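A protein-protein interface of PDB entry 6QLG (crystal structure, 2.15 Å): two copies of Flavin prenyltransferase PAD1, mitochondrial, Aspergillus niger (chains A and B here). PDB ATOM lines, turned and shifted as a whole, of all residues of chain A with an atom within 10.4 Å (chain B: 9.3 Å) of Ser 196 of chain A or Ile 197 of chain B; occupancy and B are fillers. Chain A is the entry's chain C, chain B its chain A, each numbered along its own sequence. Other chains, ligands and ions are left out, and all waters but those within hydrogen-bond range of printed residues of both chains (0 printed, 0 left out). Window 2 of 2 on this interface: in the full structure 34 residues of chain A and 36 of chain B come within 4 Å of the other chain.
Phe 190 of chain A touches Ile 201 of chain B, and with the chains exchanged Ile 201 of chain A touches Phe 190 of chain B.
Ser 196 of chain A touches Ile 197 of chain B, and with the chains exchanged Ile 197 of chain A touches Ser 196 of chain B.
Ile 197 of chain B touches its own counterpart, Ile 197 of chain A.
Ile 197 of chain A touches Leu 200 of chain B, and with the chains exchanged Leu 200 of chain A touches Ile 197 of chain B.
Of the 7 pairs that touch across the chains among the printed residues, 7 have their exchanged pair printed and touching as well.
Of the 20 printed residues of chain B, 5 touch a printed residue of chain A.
Of the 18 printed residues of chain A, 5 touch a printed residue of chain B.
Among the printed residues, 7 pairs touch across the chains.
OG of Ser 196 of chain A sits close to N of Glu 198 of chain A (3.3 Å).
The backbone NH (N) of Asp 199 of chain A is in hydrogen-bond range of the side-chain hydroxyl (OG) of Ser 196 of chain A.
The side-chain hydroxyl (OG) of Ser 204 of chain A lies within hydrogen-bond range of the backbone carbonyl oxygen (O) of Leu 200 of chain A (3.2 Å).
The side-chain hydroxyl (OG) of Ser 196 of chain B lies close to the backbone NH (N) of Glu 198 of chain B.
The side-chain hydroxyl (OG) of Ser 196 of chain B is in hydrogen-bond range of the backbone NH (N) of Asp 199 of chain B, 3.2 Å away.
The side-chain hydroxyl (OG) of Ser 204 of chain B sits at hydrogen-bond distance from the backbone carbonyl oxygen (O) of Leu 200 of chain B, 3.3 Å away.
Ile 201 of chain B touches Phe 190 of chain A (CD1 to CE1, 3.98 Å).
Ser 196 of chain A touches Ile 197 of chain B.
CD1 of Ile 197 of chain A touches O of Ser 196 of chain B, at 3.4 Å.
Ile 197 of chain A touches Ile 197 of chain B.
CD1 of Ile 197 of chain A touches CD1 of Leu 200 of chain B, at 3.7 Å.
Leu 200 of chain A touches Ile 197 of chain B (CD1 to CD1, 3.6 Å).
CE1 of Phe 190 of chain B touches CD1 of Ile 201 of chain A, 3.9 Å away.
Gly 195 of chain A touches none of the printed residues of chain B.
Ser 196 of chain A touches just one residue of chain B: Ile 197 (3.5 Å).
Of chain B, only Ser 196 (3.4 Å), Ile 197 (3.8 Å) and Leu 200 (3.7 Å) come within 4 Å of Ile 197 of chain A.
Of the printed residues of chain B, Ile 201 of chain A touches Phe 190.
Ala 189 of chain B touches none of the printed residues of chain A.
Of chain A, only Ser 196 (3.5 Å), Ile 197 (3.8 Å) and Leu 200 (3.6 Å) come within 4 Å of Ile 197 of chain B.
No residue of chain A comes within 4 Å of Asp 199 of chain B.
Of chain A, only Ile 197 (3.7 Å) comes within 4 Å of Leu 200 of chain B.
Printed residues of chain A within 4 Å of Ile 201 of chain B: Phe 190 (3.98 Å).
The nearest residue of chain B that does not touch Ser 196 of chain A is Ser 196 of chain B (6.6 Å).
The nearest residue of chain A that does not touch Ile 197 of chain B is Phe 190 of chain A (4.1 Å).
The nearest printed residue of chain B that does not touch Phe 190 of chain A is Ile 197 of chain B (4.1 Å).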
ATOM      1  N   LYS A  58     -13.429 -35.069  31.163  1.00  0.00           N
ATOM      2  CA  LYS A  58     -14.833 -34.692  31.059  1.00  0.00           C
ATOM      3  C   LYS A  58     -15.754 -35.898  31.196  1.00  0.00           C
ATOM      4  O   LYS A  58     -16.877 -35.765  31.696  1.00  0.00           O
ATOM      5  CB  LYS A  58     -15.089 -33.976  29.733  1.00  0.00           C
ATOM      6  CG  LYS A  58     -14.540 -32.558  29.683  1.00  0.00           C
ATOM      7  CD  LYS A  58     -15.520 -31.572  30.291  1.00  0.00           C
ATOM      8  CE  LYS A  58     -15.416 -30.209  29.628  1.00  0.00           C
ATOM      9  NZ  LYS A  58     -16.704 -29.469  29.710  1.00  0.00           N
ATOM     10  N   PRO A 188     -15.137 -34.154  15.688  1.00  0.00           N
ATOM     11  CA  PRO A 188     -16.058 -33.105  16.139  1.00  0.00           C
ATOM     12  C   PRO A 188     -17.347 -33.081  15.332  1.00  0.00           C
ATOM     13  O   PRO A 188     -17.371 -33.396  14.139  1.00  0.00           O
ATOM     14  CB  PRO A 188     -15.256 -31.811  15.929  1.00  0.00           C
ATOM     15  CG  PRO A 188     -13.833 -32.244  15.697  1.00  0.00           C
ATOM     16  CD  PRO A 188     -13.906 -33.607  15.098  1.00  0.00           C
ATOM     17  N   ALA A 189     -18.430 -32.693  16.001  1.00  0.00           N
ATOM     18  CA  ALA A 189     -19.740 -32.538  15.368  1.00  0.00           C
ATOM     19  C   ALA A 189     -19.969 -31.049  15.136  1.00  0.00           C
ATOM     20  O   ALA A 189     -20.593 -30.364  15.947  1.00  0.00           O
ATOM     21  CB  ALA A 189     -20.839 -33.146  16.231  1.00  0.00           C
ATOM     22  N   PHE A 190     -19.469 -30.549  14.003  1.00  0.00           N
ATOM     23  CA  PHE A 190     -19.567 -29.123  13.706  1.00  0.00           C
ATOM     24  C   PHE A 190     -21.000 -28.663  13.470  1.00  0.00           C
ATOM     25  O   PHE A 190     -21.260 -27.455  13.508  1.00  0.00           O
ATOM     26  CB  PHE A 190     -18.715 -28.777  12.484  1.00  0.00           C
ATOM     27  CG  PHE A 190     -17.240 -28.977  12.691  1.00  0.00           C
ATOM     28  CD1 PHE A 190     -16.487 -28.025  13.355  1.00  0.00           C
ATOM     29  CD2 PHE A 190     -16.605 -30.110  12.209  1.00  0.00           C
ATOM     30  CE1 PHE A 190     -15.128 -28.200  13.539  1.00  0.00           C
ATOM     31  CE2 PHE A 190     -15.244 -30.292  12.386  1.00  0.00           C
ATOM     32  CZ  PHE A 190     -14.504 -29.335  13.055  1.00  0.00           C
ATOM     33  N   TYR A 191     -21.931 -29.591  13.221  1.00  0.00           N
ATOM     34  CA  TYR A 191     -23.309 -29.206  12.934  1.00  0.00           C
ATOM     35  C   TYR A 191     -24.020 -28.624  14.148  1.00  0.00           C
ATOM     36  O   TYR A 191     -25.109 -28.059  14.000  1.00  0.00           O
ATOM     37  CB  TYR A 191     -24.083 -30.405  12.376  1.00  0.00           C
ATOM     38  CG  TYR A 191     -24.298 -31.554  13.341  1.00  0.00           C
ATOM     39  CD1 TYR A 191     -25.233 -31.476  14.371  1.00  0.00           C
ATOM     40  CD2 TYR A 191     -23.571 -32.730  13.209  1.00  0.00           C
ATOM     41  CE1 TYR A 191     -25.423 -32.531  15.245  1.00  0.00           C
ATOM     42  CE2 TYR A 191     -23.756 -33.786  14.073  1.00  0.00           C
ATOM     43  CZ  TYR A 191     -24.681 -33.683  15.087  1.00  0.00           C
ATOM     44  OH  TYR A 191     -24.862 -34.740  15.943  1.00  0.00           O
ATOM     45  N   ILE A 192     -23.445 -28.767  15.348  1.00  0.00           N
ATOM     46  CA  ILE A 192     -24.022 -28.135  16.534  1.00  0.00           C
ATOM     47  C   ILE A 192     -23.765 -26.640  16.575  1.00  0.00           C
ATOM     48  O   ILE A 192     -24.278 -25.961  17.473  1.00  0.00           O
ATOM     49  CB  ILE A 192     -23.486 -28.762  17.837  1.00  0.00           C
ATOM     50  CG1 ILE A 192     -22.021 -28.379  18.061  1.00  0.00           C
ATOM     51  CG2 ILE A 192     -23.658 -30.276  17.813  1.00  0.00           C
ATOM     52  CD1 ILE A 192     -21.447 -28.904  19.369  1.00  0.00           C
ATOM     53  N   LYS A 193     -22.993 -26.107  15.627  1.00  0.00           N
ATOM     54  CA  LYS A 193     -22.634 -24.691  15.582  1.00  0.00           C
ATOM     55  C   LYS A 193     -22.060 -24.244  16.927  1.00  0.00           C
ATOM     56  O   LYS A 193     -22.598 -23.378  17.622  1.00  0.00           O
ATOM     57  CB  LYS A 193     -23.834 -23.839  15.161  1.00  0.00           C
ATOM     58  CG  LYS A 193     -24.236 -24.052  13.707  1.00  0.00           C
ATOM     59  CD  LYS A 193     -25.160 -22.958  13.201  1.00  0.00           C
ATOM     60  CE  LYS A 193     -26.618 -23.326  13.414  1.00  0.00           C
ATOM     61  NZ  LYS A 193     -27.532 -22.220  13.006  1.00  0.00           N
ATOM     62  N   ALA A 194     -20.942 -24.871  17.284  1.00  0.00           N
ATOM     63  CA  ALA A 194     -20.337 -24.667  18.589  1.00  0.00           C
ATOM     64  C   ALA A 194     -19.653 -23.309  18.674  1.00  0.00           C
ATOM     65  O   ALA A 194     -19.199 -22.750  17.673  1.00  0.00           O
ATOM     66  CB  ALA A 194     -19.325 -25.773  18.880  1.00  0.00           C
ATOM     67  N   GLY A 195     -19.574 -22.783  19.892  1.00  0.00           N
ATOM     68  CA  GLY A 195     -18.904 -21.532  20.159  1.00  0.00           C
ATOM     69  C   GLY A 195     -17.521 -21.653  20.754  1.00  0.00           C
ATOM     70  O   GLY A 195     -16.880 -20.627  21.000  1.00  0.00           O
ATOM     71  N   SER A 196     -17.035 -22.871  20.987  1.00  0.00           N
ATOM     72  CA  SER A 196     -15.732 -23.081  21.607  1.00  0.00           C
ATOM     73  C   SER A 196     -15.353 -24.548  21.462  1.00  0.00           C
ATOM     74  O   SER A 196     -16.177 -25.393  21.103  1.00  0.00           O
ATOM     75  CB  SER A 196     -15.737 -22.672  23.081  1.00  0.00           C
ATOM     76  OG  SER A 196     -16.412 -23.640  23.866  1.00  0.00           O
ATOM     77  N   ILE A 197     -14.083 -24.837  21.757  1.00  0.00           N
ATOM     78  CA  ILE A 197     -13.607 -26.218  21.762  1.00  0.00           C
ATOM     79  C   ILE A 197     -14.370 -27.037  22.795  1.00  0.00           C
ATOM     80  O   ILE A 197     -14.696 -28.209  22.566  1.00  0.00           O
ATOM     81  CB  ILE A 197     -12.088 -26.254  22.019  1.00  0.00           C
ATOM     82  CG1 ILE A 197     -11.325 -25.684  20.821  1.00  0.00           C
ATOM     83  CG2 ILE A 197     -11.616 -27.671  22.333  1.00  0.00           C
ATOM     84  CD1 ILE A 197      -9.881 -25.343  21.133  1.00  0.00           C
ATOM     85  N   GLU A 198     -14.683 -26.426  23.941  1.00  0.00           N
ATOM     86  CA  GLU A 198     -15.354 -27.156  25.012  1.00  0.00           C
ATOM     87  C   GLU A 198     -16.746 -27.612  24.595  1.00  0.00           C
ATOM     88  O   GLU A 198     -17.202 -28.682  25.012  1.00  0.00           O
ATOM     89  CB  GLU A 198     -15.431 -26.293  26.271  1.00  0.00           C
ATOM     90  CG  GLU A 198     -15.739 -27.088  27.528  1.00  0.00           C
ATOM     91  CD  GLU A 198     -15.815 -26.225  28.772  1.00  0.00           C
ATOM     92  OE1 GLU A 198     -15.936 -24.990  28.636  1.00  0.00           O
ATOM     93  OE2 GLU A 198     -15.760 -26.786  29.888  1.00  0.00           O
ATOM     94  N   ASP A 199     -17.441 -26.811  23.782  1.00  0.00           N
ATOM     95  CA  ASP A 199     -18.751 -27.224  23.288  1.00  0.00           C
ATOM     96  C   ASP A 199     -18.651 -28.512  22.483  1.00  0.00           C
ATOM     97  O   ASP A 199     -19.475 -29.421  22.642  1.00  0.00           O
ATOM     98  CB  ASP A 199     -19.374 -26.120  22.435  1.00  0.00           C
ATOM     99  CG  ASP A 199     -19.848 -24.935  23.257  1.00  0.00           C
ATOM    100  OD1 ASP A 199     -19.981 -25.072  24.491  1.00  0.00           O
ATOM    101  OD2 ASP A 199     -20.097 -23.866  22.660  1.00  0.00           O
ATOM    102  N   LEU A 200     -17.646 -28.606  21.610  1.00  0.00           N
ATOM    103  CA  LEU A 200     -17.484 -29.799  20.785  1.00  0.00           C
ATOM    104  C   LEU A 200     -17.076 -31.002  21.629  1.00  0.00           C
ATOM    105  O   LEU A 200     -17.543 -32.121  21.386  1.00  0.00           O
ATOM    106  CB  LEU A 200     -16.469 -29.519  19.675  1.00  0.00           C
ATOM    107  CG  LEU A 200     -16.994 -28.533  18.619  1.00  0.00           C
ATOM    108  CD1 LEU A 200     -15.895 -27.966  17.728  1.00  0.00           C
ATOM    109  CD2 LEU A 200     -18.068 -29.197  17.768  1.00  0.00           C
ATOM    110  N   ILE A 201     -16.223 -30.791  22.635  1.00  0.00           N
ATOM    111  CA  ILE A 201     -15.847 -31.884  23.529  1.00  0.00           C
ATOM    112  C   ILE A 201     -17.059 -32.367  24.317  1.00  0.00           C
ATOM    113  O   ILE A 201     -17.275 -33.576  24.473  1.00  0.00           O
ATOM    114  CB  ILE A 201     -14.702 -31.447  24.462  1.00  0.00           C
ATOM    115  CG1 ILE A 201     -13.434 -31.158  23.655  1.00  0.00           C
ATOM    116  CG2 ILE A 201     -14.429 -32.510  25.519  1.00  0.00           C
ATOM    117  CD1 ILE A 201     -12.267 -30.700  24.499  1.00  0.00           C
ATOM    118  N   ASP A 202     -17.867 -31.431  24.826  1.00  0.00           N
ATOM    119  CA  ASP A 202     -19.063 -31.805  25.575  1.00  0.00           C
ATOM    120  C   ASP A 202     -19.997 -32.658  24.730  1.00  0.00           C
ATOM    121  O   ASP A 202     -20.593 -33.622  25.227  1.00  0.00           O
ATOM    122  CB  ASP A 202     -19.792 -30.552  26.068  1.00  0.00           C
ATOM    123  CG  ASP A 202     -19.092 -29.888  27.240  1.00  0.00           C
ATOM    124  OD1 ASP A 202     -18.213 -30.527  27.853  1.00  0.00           O
ATOM    125  OD2 ASP A 202     -19.424 -28.722  27.546  1.00  0.00           O
ATOM    126  N   GLN A 203     -20.140 -32.318  23.447  1.00  0.00           N
ATOM    127  CA  GLN A 203     -21.003 -33.100  22.569  1.00  0.00           C
ATOM    128  C   GLN A 203     -20.445 -34.503  22.358  1.00  0.00           C
ATOM    129  O   GLN A 203     -21.197 -35.484  22.377  1.00  0.00           O
ATOM    130  CB  GLN A 203     -21.188 -32.380  21.231  1.00  0.00           C
ATOM    131  CG  GLN A 203     -22.341 -32.925  20.394  1.00  0.00           C
ATOM    132  CD  GLN A 203     -21.929 -34.057  19.464  1.00  0.00           C
ATOM    133  OE1 GLN A 203     -20.763 -34.450  19.425  1.00  0.00           O
ATOM    134  NE2 GLN A 203     -22.890 -34.592  18.716  1.00  0.00           N
ATOM    135  N   SER A 204     -19.129 -34.622  22.164  1.00  0.00           N
ATOM    136  CA  SER A 204     -18.519 -35.939  21.999  1.00  0.00           C
ATOM    137  C   SER A 204     -18.707 -36.787  23.250  1.00  0.00           C
ATOM    138  O   SER A 204     -19.070 -37.968  23.166  1.00  0.00           O
ATOM    139  CB  SER A 204     -17.033 -35.799  21.662  1.00  0.00           C
ATOM    140  OG  SER A 204     -16.848 -35.067  20.465  1.00  0.00           O
ATOM    141  N   MET B  54     -16.084 -26.706   7.041  1.00  0.00           N
ATOM    142  CA  MET B  54     -14.943 -25.803   7.180  1.00  0.00           C
ATOM    143  C   MET B  54     -13.623 -26.505   6.892  1.00  0.00           C
ATOM    144  O   MET B  54     -12.654 -25.854   6.480  1.00  0.00           O
ATOM    145  CB  MET B  54     -14.923 -25.188   8.581  1.00  0.00           C
ATOM    146  CG  MET B  54     -13.953 -24.020   8.739  1.00  0.00           C
ATOM    147  SD  MET B  54     -14.226 -22.662   7.573  1.00  0.00           S
ATOM    148  CE  MET B  54     -15.959 -22.348   7.838  1.00  0.00           C
ATOM    149  N   LEU B  55     -13.558 -27.824   7.097  1.00  0.00           N
ATOM    150  CA  LEU B  55     -12.347 -28.562   6.749  1.00  0.00           C
ATOM    151  C   LEU B  55     -12.050 -28.458   5.258  1.00  0.00           C
ATOM    152  O   LEU B  55     -10.903 -28.226   4.859  1.00  0.00           O
ATOM    153  CB  LEU B  55     -12.481 -30.029   7.167  1.00  0.00           C
ATOM    154  CG  LEU B  55     -12.657 -30.330   8.657  1.00  0.00           C
ATOM    155  CD1 LEU B  55     -12.890 -31.818   8.876  1.00  0.00           C
ATOM    156  CD2 LEU B  55     -11.453 -29.853   9.450  1.00  0.00           C
ATOM    157  N   LYS B  58     -11.040 -24.770   4.287  1.00  0.00           N
ATOM    158  CA  LYS B  58      -9.670 -24.426   4.650  1.00  0.00           C
ATOM    159  C   LYS B  58      -8.651 -25.186   3.809  1.00  0.00           C
ATOM    160  O   LYS B  58      -7.528 -24.704   3.622  1.00  0.00           O
ATOM    161  CB  LYS B  58      -9.442 -24.683   6.138  1.00  0.00           C
ATOM    162  CG  LYS B  58     -10.218 -23.733   7.035  1.00  0.00           C
ATOM    163  CD  LYS B  58      -9.493 -23.486   8.343  1.00  0.00           C
ATOM    164  CE  LYS B  58      -9.692 -22.059   8.820  1.00  0.00           C
ATOM    165  NZ  LYS B  58      -8.390 -21.390   9.087  1.00  0.00           N
ATOM    166  N   PRO B 188      -8.971 -34.231  16.514  1.00  0.00           N
ATOM    167  CA  PRO B 188      -8.139 -33.072  16.869  1.00  0.00           C
ATOM    168  C   PRO B 188      -6.847 -33.488  17.553  1.00  0.00           C
ATOM    169  O   PRO B 188      -6.813 -34.443  18.333  1.00  0.00           O
ATOM    170  CB  PRO B 188      -9.034 -32.266  17.822  1.00  0.00           C
ATOM    171  CG  PRO B 188     -10.401 -32.895  17.734  1.00  0.00           C
ATOM    172  CD  PRO B 188     -10.184 -34.314  17.340  1.00  0.00           C
ATOM    173  N   ALA B 189      -5.777 -32.752  17.254  1.00  0.00           N
ATOM    174  CA  ALA B 189      -4.479 -32.956  17.896  1.00  0.00           C
ATOM    175  C   ALA B 189      -4.379 -31.980  19.061  1.00  0.00           C
ATOM    176  O   ALA B 189      -3.853 -30.873  18.934  1.00  0.00           O
ATOM    177  CB  ALA B 189      -3.345 -32.766  16.899  1.00  0.00           C
ATOM    178  N   PHE B 190      -4.890 -32.399  20.222  1.00  0.00           N
ATOM    179  CA  PHE B 190      -4.960 -31.505  21.372  1.00  0.00           C
ATOM    180  C   PHE B 190      -3.589 -31.143  21.930  1.00  0.00           C
ATOM    181  O   PHE B 190      -3.482 -30.162  22.674  1.00  0.00           O
ATOM    182  CB  PHE B 190      -5.816 -32.130  22.474  1.00  0.00           C
ATOM    183  CG  PHE B 190      -7.268 -32.272  22.110  1.00  0.00           C
ATOM    184  CD1 PHE B 190      -8.127 -31.189  22.197  1.00  0.00           C
ATOM    185  CD2 PHE B 190      -7.773 -33.486  21.679  1.00  0.00           C
ATOM    186  CE1 PHE B 190      -9.464 -31.318  21.865  1.00  0.00           C
ATOM    187  CE2 PHE B 190      -9.108 -33.623  21.347  1.00  0.00           C
ATOM    188  CZ  PHE B 190      -9.955 -32.536  21.439  1.00  0.00           C
ATOM    189  N   ILE B 192      -1.188 -29.691  20.614  1.00  0.00           N
ATOM    190  CA  ILE B 192      -0.702 -28.389  20.170  1.00  0.00           C
ATOM    191  C   ILE B 192      -1.132 -27.262  21.094  1.00  0.00           C
ATOM    192  O   ILE B 192      -0.686 -26.123  20.911  1.00  0.00           O
ATOM    193  CB  ILE B 192      -1.170 -28.076  18.734  1.00  0.00           C
ATOM    194  CG1 ILE B 192      -2.655 -27.705  18.720  1.00  0.00           C
ATOM    195  CG2 ILE B 192      -0.895 -29.255  17.811  1.00  0.00           C
ATOM    196  CD1 ILE B 192      -3.138 -27.176  17.382  1.00  0.00           C
ATOM    197  N   LYS B 193      -1.983 -27.552  22.078  1.00  0.00           N
ATOM    198  CA  LYS B 193      -2.484 -26.565  23.034  1.00  0.00           C
ATOM    199  C   LYS B 193      -3.115 -25.377  22.304  1.00  0.00           C
ATOM    200  O   LYS B 193      -2.625 -24.248  22.327  1.00  0.00           O
ATOM    201  CB  LYS B 193      -1.367 -26.116  23.983  1.00  0.00           C
ATOM    202  CG  LYS B 193      -0.807 -27.244  24.844  1.00  0.00           C
ATOM    203  CD  LYS B 193       0.194 -26.726  25.862  1.00  0.00           C
ATOM    204  CE  LYS B 193       1.619 -27.049  25.445  1.00  0.00           C
ATOM    205  NZ  LYS B 193       2.600 -26.698  26.509  1.00  0.00           N
ATOM    206  N   ALA B 194      -4.227 -25.680  21.644  1.00  0.00           N
ATOM    207  CA  ALA B 194      -4.903 -24.707  20.803  1.00  0.00           C
ATOM    208  C   ALA B 194      -5.710 -23.723  21.638  1.00  0.00           C
ATOM    209  O   ALA B 194      -6.271 -24.068  22.681  1.00  0.00           O
ATOM    210  CB  ALA B 194      -5.822 -25.412  19.807  1.00  0.00           C
ATOM    211  N   GLY B 195      -5.769 -22.483  21.160  1.00  0.00           N
ATOM    212  CA  GLY B 195      -6.595 -21.457  21.750  1.00  0.00           C
ATOM    213  C   GLY B 195      -7.919 -21.234  21.056  1.00  0.00           C
ATOM    214  O   GLY B 195      -8.686 -20.363  21.477  1.00  0.00           O
ATOM    215  N   SER B 196      -8.214 -21.997  20.006  1.00  0.00           N
ATOM    216  CA  SER B 196      -9.447 -21.828  19.249  1.00  0.00           C
ATOM    217  C   SER B 196      -9.706 -23.088  18.438  1.00  0.00           C
ATOM    218  O   SER B 196      -8.805 -23.903  18.217  1.00  0.00           O
ATOM    219  CB  SER B 196      -9.374 -20.611  18.323  1.00  0.00           C
ATOM    220  OG  SER B 196      -8.443 -20.834  17.279  1.00  0.00           O
ATOM    221  N   ILE B 197     -10.957 -23.232  17.995  1.00  0.00           N
ATOM    222  CA  ILE B 197     -11.310 -24.328  17.095  1.00  0.00           C
ATOM    223  C   ILE B 197     -10.480 -24.250  15.822  1.00  0.00           C
ATOM    224  O   ILE B 197      -9.999 -25.268  15.307  1.00  0.00           O
ATOM    225  CB  ILE B 197     -12.819 -24.295  16.787  1.00  0.00           C
ATOM    226  CG1 ILE B 197     -13.635 -24.658  18.029  1.00  0.00           C
ATOM    227  CG2 ILE B 197     -13.155 -25.226  15.629  1.00  0.00           C
ATOM    228  CD1 ILE B 197     -15.124 -24.424  17.857  1.00  0.00           C
ATOM    229  N   GLU B 198     -10.285 -23.033  15.304  1.00  0.00           N
ATOM    230  CA  GLU B 198      -9.568 -22.853  14.048  1.00  0.00           C
ATOM    231  C   GLU B 198      -8.128 -23.343  14.137  1.00  0.00           C
ATOM    232  O   GLU B 198      -7.583 -23.842  13.146  1.00  0.00           O
ATOM    233  CB  GLU B 198      -9.612 -21.380  13.638  1.00  0.00           C
ATOM    234  CG  GLU B 198      -8.945 -21.078  12.311  1.00  0.00           C
ATOM    235  CD  GLU B 198      -9.113 -19.632  11.888  1.00  0.00           C
ATOM    236  OE1 GLU B 198      -9.210 -18.757  12.776  1.00  0.00           O
ATOM    237  OE2 GLU B 198      -9.149 -19.369  10.667  1.00  0.00           O
ATOM    238  N   ASP B 199      -7.494 -23.208  15.306  1.00  0.00           N
ATOM    239  CA  ASP B 199      -6.137 -23.721  15.476  1.00  0.00           C
ATOM    240  C   ASP B 199      -6.088 -25.228  15.262  1.00  0.00           C
ATOM    241  O   ASP B 199      -5.188 -25.740  14.587  1.00  0.00           O
ATOM    242  CB  ASP B 199      -5.608 -23.376  16.867  1.00  0.00           C
ATOM    243  CG  ASP B 199      -5.294 -21.904  17.027  1.00  0.00           C
ATOM    244  OD1 ASP B 199      -5.109 -21.213  16.002  1.00  0.00           O
ATOM    245  OD2 ASP B 199      -5.230 -21.442  18.185  1.00  0.00           O
ATOM    246  N   LEU B 200      -7.046 -25.955  15.838  1.00  0.00           N
ATOM    247  CA  LEU B 200      -7.082 -27.401  15.654  1.00  0.00           C
ATOM    248  C   LEU B 200      -7.386 -27.761  14.205  1.00  0.00           C
ATOM    249  O   LEU B 200      -6.797 -28.700  13.657  1.00  0.00           O
ATOM    250  CB  LEU B 200      -8.104 -28.016  16.610  1.00  0.00           C
ATOM    251  CG  LEU B 200      -7.713 -27.919  18.089  1.00  0.00           C
ATOM    252  CD1 LEU B 200      -8.897 -28.155  19.015  1.00  0.00           C
ATOM    253  CD2 LEU B 200      -6.578 -28.887  18.413  1.00  0.00           C
ATOM    254  N   ILE B 201      -8.283 -27.009  13.560  1.00  0.00           N
ATOM    255  CA  ILE B 201      -8.583 -27.250  12.151  1.00  0.00           C
ATOM    256  C   ILE B 201      -7.342 -27.023  11.295  1.00  0.00           C
ATOM    257  O   ILE B 201      -7.051 -27.805  10.381  1.00  0.00           O
ATOM    258  CB  ILE B 201      -9.753 -26.360  11.689  1.00  0.00           C
ATOM    259  CG1 ILE B 201     -11.039 -26.727  12.429  1.00  0.00           C
ATOM    260  CG2 ILE B 201      -9.964 -26.497  10.189  1.00  0.00           C
ATOM    261  CD1 ILE B 201     -12.250 -25.944  11.962  1.00  0.00           C
ATOM    262  N   ASP B 202      -6.591 -25.955  11.581  1.00  0.00           N
ATOM    263  CA  ASP B 202      -5.397 -25.649  10.798  1.00  0.00           C
ATOM    264  C   ASP B 202      -4.377 -26.778  10.876  1.00  0.00           C
ATOM    265  O   ASP B 202      -3.720 -27.103   9.880  1.00  0.00           O
ATOM    266  CB  ASP B 202      -4.773 -24.337  11.279  1.00  0.00           C
ATOM    267  CG  ASP B 202      -5.592 -23.118  10.891  1.00  0.00           C
ATOM    268  OD1 ASP B 202      -6.379 -23.202   9.923  1.00  0.00           O
ATOM    269  OD2 ASP B 202      -5.448 -22.072  11.559  1.00  0.00           O
ATOM    270  N   GLN B 203      -4.225 -27.383  12.055  1.00  0.00           N
ATOM    271  CA  GLN B 203      -3.301 -28.504  12.190  1.00  0.00           C
ATOM    272  C   GLN B 203      -3.782 -29.714  11.397  1.00  0.00           C
ATOM    273  O   GLN B 203      -2.987 -30.370  10.714  1.00  0.00           O
ATOM    274  CB  GLN B 203      -3.120 -28.857  13.667  1.00  0.00           C
ATOM    275  CG  GLN B 203      -1.959 -29.799  13.950  1.00  0.00           C
ATOM    276  CD  GLN B 203      -2.373 -31.261  13.949  1.00  0.00           C
ATOM    277  OE1 GLN B 203      -3.553 -31.584  13.799  1.00  0.00           O
ATOM    278  NE2 GLN B 203      -1.404 -32.152  14.128  1.00  0.00           N
ATOM    279  N   SER B 204      -5.083 -30.020  11.468  1.00  0.00           N
ATOM    280  CA  SER B 204      -5.622 -31.142  10.704  1.00  0.00           C
ATOM    281  C   SER B 204      -5.431 -30.931   9.208  1.00  0.00           C
ATOM    282  O   SER B 204      -5.042 -31.857   8.488  1.00  0.00           O
ATOM    283  CB  SER B 204      -7.104 -31.339  11.026  1.00  0.00           C
ATOM    284  OG  SER B 204      -7.296 -31.685  12.386  1.00  0.00           O
ATOM    285  N   VAL B 205      -5.700 -29.715   8.724  1.00  0.00           N
ATOM    286  CA  VAL B 205      -5.535 -29.424   7.301  1.00  0.00           C
ATOM    287  C   VAL B 205      -4.075 -29.577   6.895  1.00  0.00           C
ATOM    288  O   VAL B 205      -3.765 -30.105   5.819  1.00  0.00           O
ATOM    289  CB  VAL B 205      -6.074 -28.017   6.981  1.00  0.00           C
ATOM    290  CG1 VAL B 205      -5.627 -27.571   5.597  1.00  0.00           C
ATOM    291  CG2 VAL B 205      -7.593 -27.998   7.091  1.00  0.00           C
